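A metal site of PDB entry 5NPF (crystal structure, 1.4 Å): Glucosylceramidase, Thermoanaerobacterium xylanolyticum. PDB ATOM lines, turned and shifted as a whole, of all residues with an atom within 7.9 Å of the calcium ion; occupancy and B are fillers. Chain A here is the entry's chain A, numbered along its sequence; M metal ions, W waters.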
ATOM      1  N   LYS A 556       4.863 -15.945  -0.756  1.00  0.00           N
ATOM      2  CA  LYS A 556       4.317 -17.318  -0.741  1.00  0.00           C
ATOM      3  C   LYS A 556       5.179 -18.313   0.079  1.00  0.00           C
ATOM      4  O   LYS A 556       4.645 -19.233   0.700  1.00  0.00           O
ATOM      5  CB  LYS A 556       4.203 -17.841  -2.162  1.00  0.00           C
ATOM      6  CG  LYS A 556       3.621 -19.251  -2.325  1.00  0.00           C
ATOM      7  CD  LYS A 556       2.212 -19.378  -1.778  1.00  0.00           C
ATOM      8  CE  LYS A 556       1.363 -20.370  -2.523  1.00  0.00           C
ATOM      9  NZ  LYS A 556       1.871 -21.742  -2.532  1.00  0.00           N
ATOM     10  N   MET A 558       6.391 -17.756   2.839  1.00  0.00           N
ATOM     11  CA  MET A 558       6.040 -17.603   4.248  1.00  0.00           C
ATOM     12  C   MET A 558       4.768 -18.327   4.669  1.00  0.00           C
ATOM     13  O   MET A 558       4.334 -18.251   5.823  1.00  0.00           O
ATOM     14  CB  MET A 558       6.005 -16.125   4.614  1.00  0.00           C
ATOM     15  CG  MET A 558       7.354 -15.487   4.349  1.00  0.00           C
ATOM     16  SD  MET A 558       7.297 -13.712   4.588  1.00  0.00           S
ATOM     17  CE  MET A 558       9.008 -13.278   4.328  1.00  0.00           C
ATOM     18  N   ASP A 559       4.218 -19.101   3.745  1.00  0.00           N
ATOM     19  CA  ASP A 559       3.124 -20.038   4.042  1.00  0.00           C
ATOM     20  C   ASP A 559       3.685 -21.333   4.543  1.00  0.00           C
ATOM     21  O   ASP A 559       3.955 -22.234   3.764  1.00  0.00           O
ATOM     22  CB  ASP A 559       2.296 -20.282   2.778  1.00  0.00           C
ATOM     23  CG  ASP A 559       1.188 -21.304   2.987  1.00  0.00           C
ATOM     24  OD1 ASP A 559       0.754 -21.480   4.164  1.00  0.00           O
ATOM     25  OD2 ASP A 559       0.746 -21.916   1.984  1.00  0.00           O
ATOM     26  N   LYS A 560       3.814 -21.466   5.849  1.00  0.00           N
ATOM     27  CA  LYS A 560       4.417 -22.684   6.425  1.00  0.00           C
ATOM     28  C   LYS A 560       3.447 -23.860   6.636  1.00  0.00           C
ATOM     29  O   LYS A 560       3.892 -24.926   6.913  1.00  0.00           O
ATOM     30  CB  LYS A 560       5.142 -22.391   7.732  1.00  0.00           C
ATOM     31  CG  LYS A 560       6.119 -21.233   7.663  1.00  0.00           C
ATOM     32  CD  LYS A 560       7.208 -21.400   6.601  1.00  0.00           C
ATOM     33  CE  LYS A 560       8.316 -20.367   6.775  1.00  0.00           C
ATOM     34  NZ  LYS A 560       9.657 -20.973   6.562  1.00  0.00           N
ATOM     35  N   ASP A 561       2.134 -23.650   6.446  1.00  0.00           N
ATOM     36  CA  ASP A 561       1.245 -24.821   6.703  1.00  0.00           C
ATOM     37  C   ASP A 561       0.490 -25.173   5.404  1.00  0.00           C
ATOM     38  O   ASP A 561      -0.414 -26.004   5.444  1.00  0.00           O
ATOM     39  CB  ASP A 561       0.242 -24.569   7.837  1.00  0.00           C
ATOM     40  CG  ASP A 561      -0.717 -23.419   7.537  1.00  0.00           C
ATOM     41  OD1 ASP A 561      -0.433 -22.610   6.624  1.00  0.00           O
ATOM     42  OD2 ASP A 561      -1.774 -23.311   8.191  1.00  0.00           O
ATOM     43  N   ASN A 562       0.914 -24.622   4.278  1.00  0.00           N
ATOM     44  CA  ASN A 562       0.371 -24.982   2.972  1.00  0.00           C
ATOM     45  C   ASN A 562      -1.159 -24.795   2.782  1.00  0.00           C
ATOM     46  O   ASN A 562      -1.808 -25.557   2.055  1.00  0.00           O
ATOM     47  CB  ASN A 562       0.796 -26.430   2.592  1.00  0.00           C
ATOM     48  CG  ASN A 562       1.014 -26.587   1.109  1.00  0.00           C
ATOM     49  OD1 ASN A 562       1.673 -25.773   0.471  1.00  0.00           O
ATOM     50  ND2 ASN A 562       0.430 -27.638   0.541  1.00  0.00           N
ATOM     51  N   ASP A 563      -1.710 -23.752   3.408  1.00  0.00           N
ATOM     52  CA  ASP A 563      -3.104 -23.352   3.126  1.00  0.00           C
ATOM     53  C   ASP A 563      -3.147 -22.312   2.004  1.00  0.00           C
ATOM     54  O   ASP A 563      -4.199 -21.799   1.683  1.00  0.00           O
ATOM     55  CB  ASP A 563      -3.843 -22.905   4.393  1.00  0.00           C
ATOM     56  CG  ASP A 563      -3.409 -21.536   4.928  1.00  0.00           C
ATOM     57  OD1 ASP A 563      -2.348 -20.988   4.520  1.00  0.00           O
ATOM     58  OD2 ASP A 563      -4.135 -21.010   5.798  1.00  0.00           O
ATOM     59  N   GLY A 564      -1.986 -21.958   1.441  1.00  0.00           N
ATOM     60  CA  GLY A 564      -1.914 -21.015   0.331  1.00  0.00           C
ATOM     61  C   GLY A 564      -1.797 -19.542   0.744  1.00  0.00           C
ATOM     62  O   GLY A 564      -1.747 -18.668  -0.118  1.00  0.00           O
ATOM     63  N   ILE A 565      -1.698 -19.297   2.041  1.00  0.00           N
ATOM     64  CA  ILE A 565      -1.689 -17.926   2.606  1.00  0.00           C
ATOM     65  C   ILE A 565      -0.436 -17.748   3.484  1.00  0.00           C
ATOM     66  O   ILE A 565      -0.121 -18.616   4.279  1.00  0.00           O
ATOM     67  CB  ILE A 565      -2.944 -17.664   3.463  1.00  0.00           C
ATOM     68  CG1 ILE A 565      -4.208 -18.031   2.681  1.00  0.00           C
ATOM     69  CG2 ILE A 565      -2.972 -16.201   3.891  1.00  0.00           C
ATOM     70  CD1 ILE A 565      -5.479 -18.054   3.504  1.00  0.00           C
ATOM     71  N   PRO A 566       0.273 -16.624   3.368  1.00  0.00           N
ATOM     72  CA  PRO A 566       1.412 -16.407   4.270  1.00  0.00           C
ATOM     73  C   PRO A 566       0.933 -16.414   5.722  1.00  0.00           C
ATOM     74  O   PRO A 566      -0.165 -15.940   6.007  1.00  0.00           O
ATOM     75  CB  PRO A 566       1.937 -15.038   3.886  1.00  0.00           C
ATOM     76  CG  PRO A 566       0.827 -14.390   3.113  1.00  0.00           C
ATOM     77  CD  PRO A 566       0.110 -15.508   2.421  1.00  0.00           C
ATOM     78  N   ASP A 567       1.743 -16.976   6.623  1.00  0.00           N
ATOM     79  CA  ASP A 567       1.412 -17.078   8.055  1.00  0.00           C
ATOM     80  C   ASP A 567       1.962 -15.926   8.868  1.00  0.00           C
ATOM     81  O   ASP A 567       3.191 -15.715   8.919  1.00  0.00           O
ATOM     82  CB  ASP A 567       1.976 -18.346   8.702  1.00  0.00           C
ATOM     83  CG  ASP A 567       1.192 -19.565   8.342  1.00  0.00           C
ATOM     84  OD1 ASP A 567       1.339 -19.975   7.168  1.00  0.00           O
ATOM     85  OD2 ASP A 567       0.454 -20.116   9.226  1.00  0.00           O
ATOM     86  N   ASN A 568       1.082 -15.229   9.581  1.00  0.00           N
ATOM     87  CA  ASN A 568       1.557 -14.285  10.577  1.00  0.00           C
ATOM     88  C   ASN A 568       2.159 -15.131  11.720  1.00  0.00           C
ATOM     89  O   ASN A 568       1.682 -16.201  12.091  1.00  0.00           O
ATOM     90  CB  ASN A 568       0.435 -13.394  11.078  1.00  0.00           C
ATOM     91  CG  ASN A 568      -0.051 -12.393  10.018  1.00  0.00           C
ATOM     92  OD1 ASN A 568      -1.081 -12.629   9.385  1.00  0.00           O
ATOM     93  ND2 ASN A 568       0.671 -11.247   9.882  1.00  0.00           N
ATOM     94  N   GLY A 583      -1.095 -16.960  12.518  1.00  0.00           N
ATOM     95  CA  GLY A 583      -1.757 -17.867  11.607  1.00  0.00           C
ATOM     96  C   GLY A 583      -2.217 -17.144  10.357  1.00  0.00           C
ATOM     97  O   GLY A 583      -1.481 -16.293   9.832  1.00  0.00           O
ATOM     98  N   THR A 584      -3.447 -17.426   9.888  1.00  0.00           N
ATOM     99  CA  THR A 584      -4.051 -16.590   8.856  1.00  0.00           C
ATOM    100  C   THR A 584      -4.787 -15.435   9.521  1.00  0.00           C
ATOM    101  O   THR A 584      -5.625 -15.670  10.399  1.00  0.00           O
ATOM    102  CB  THR A 584      -5.000 -17.391   7.982  1.00  0.00           C
ATOM    103  OG1 THR A 584      -4.249 -18.385   7.264  1.00  0.00           O
ATOM    104  CG2 THR A 584      -5.678 -16.511   6.994  1.00  0.00           C
ATOM    105  N   ASN A 625      -9.625 -21.213   1.420  1.00  0.00           N
ATOM    106  CA  ASN A 625      -9.142 -21.416   2.765  1.00  0.00           C
ATOM    107  C   ASN A 625      -9.361 -20.196   3.650  1.00  0.00           C
ATOM    108  O   ASN A 625      -9.689 -20.342   4.809  1.00  0.00           O
ATOM    109  CB  ASN A 625      -7.677 -21.877   2.783  1.00  0.00           C
ATOM    110  CG  ASN A 625      -7.552 -23.304   2.292  1.00  0.00           C
ATOM    111  OD1 ASN A 625      -8.509 -24.082   2.452  1.00  0.00           O
ATOM    112  ND2 ASN A 625      -6.451 -23.638   1.646  1.00  0.00           N
ATOM    113  N   GLU A 629     -11.437 -20.558   7.076  1.00  0.00           N
ATOM    114  CA  GLU A 629     -10.708 -20.302   8.326  1.00  0.00           C
ATOM    115  C   GLU A 629     -11.284 -19.164   9.148  1.00  0.00           C
ATOM    116  O   GLU A 629     -11.196 -19.175  10.383  1.00  0.00           O
ATOM    117  CB  GLU A 629      -9.246 -20.032   8.012  1.00  0.00           C
ATOM    118  CG  GLU A 629      -8.426 -21.228   7.601  1.00  0.00           C
ATOM    119  CD  GLU A 629      -7.092 -20.874   6.974  1.00  0.00           C
ATOM    120  OE1 GLU A 629      -6.656 -19.744   7.128  1.00  0.00           O
ATOM    121  OE2 GLU A 629      -6.468 -21.782   6.342  1.00  0.00           O
ATOM    122  N   THR A 640      -6.480 -16.745  13.031  1.00  0.00           N
ATOM    123  CA  THR A 640      -6.824 -18.125  13.368  1.00  0.00           C
ATOM    124  C   THR A 640      -6.224 -18.666  14.672  1.00  0.00           C
ATOM    125  O   THR A 640      -6.693 -19.686  15.169  1.00  0.00           O
ATOM    126  CB  THR A 640      -6.423 -19.094  12.244  1.00  0.00           C
ATOM    127  OG1 THR A 640      -5.024 -18.962  11.957  1.00  0.00           O
ATOM    128  CG2 THR A 640      -7.213 -18.846  11.001  1.00  0.00           C
ATOM    129  N   GLU A 641      -5.195 -18.000  15.226  1.00  0.00           N
ATOM    130  CA  GLU A 641      -4.411 -18.600  16.348  1.00  0.00           C
ATOM    131  C   GLU A 641      -4.180 -17.729  17.581  1.00  0.00           C
ATOM    132  O   GLU A 641      -3.667 -18.248  18.585  1.00  0.00           O
ATOM    133  CB  GLU A 641      -3.060 -19.141  15.836  1.00  0.00           C
ATOM    134  CG  GLU A 641      -3.232 -20.272  14.814  1.00  0.00           C
ATOM    135  CD  GLU A 641      -1.915 -20.774  14.229  1.00  0.00           C
ATOM    136  OE1 GLU A 641      -0.873 -20.717  14.918  1.00  0.00           O
ATOM    137  OE2 GLU A 641      -1.916 -21.288  13.071  1.00  0.00           O
HETATM  138 CA    CA M   1      -0.578 -20.372   5.821  1.00  0.00          CA
HETATM  139  O   HOH W   1      -1.861 -20.717   7.868  1.00  0.00           O
HETATM  140  O   HOH W   2      -1.628 -18.528   6.873  1.00  0.00           O
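The calcium ion is bound by the side-chain carboxylate (OD1) of Asp 563 (2.3 Å), water W2 (2.4 Å), the side-chain carboxylate (OD1) of Asp 567 (2.4 Å), the backbone carbonyl oxygen (O) of Ile 565 (2.4 Å), the side-chain carboxylate (OD1) of Asp 561 (2.4 Å), the side-chain carboxylate (OD1) of Asp 559 (2.4 Å) and water W1 (2.4 Å). The calcium ion has seven donor atoms within binding distance.
N of Asp 567 lies within hydrogen-bond range of O of Met 558 (3.0 Å). The side-chain carboxylate (OD2) of Asp 563 sits close to the side-chain carboxylate (OE2) of Glu 629. The side-chain carboxylate (OD2) of Asp 563 lies within hydrogen-bond range of the side-chain hydroxyl (OG1) of Thr 584, at 3.0 Å. N of Asn 562 lies close to OD1 of Asp 559. The side-chain carboxylate (OD1) of Asp 567 sits close to the backbone NH (N) of Lys 560. The side-chain carboxylate of Asp 559 lies within hydrogen-bond range of the backbone NH of Gly 564 (2.8 Å). The side-chain amide nitrogen (ND2) of Asn 625 is in hydrogen-bond range of the backbone carbonyl oxygen (O) of Asp 563 (2.9 Å).
Five residues have an atom within 4 Å of the calcium ion: Asp 559, Asp 561, Asp 563, Ile 565 and Asp 567. The nearest printed residue that does not touch the calcium ion is Pro 566 (4.2 Å).
Water W2 bridges the side-chain hydroxyl (OG1) of Thr 584 and the backbone carbonyl oxygen (O) of Pro 566.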
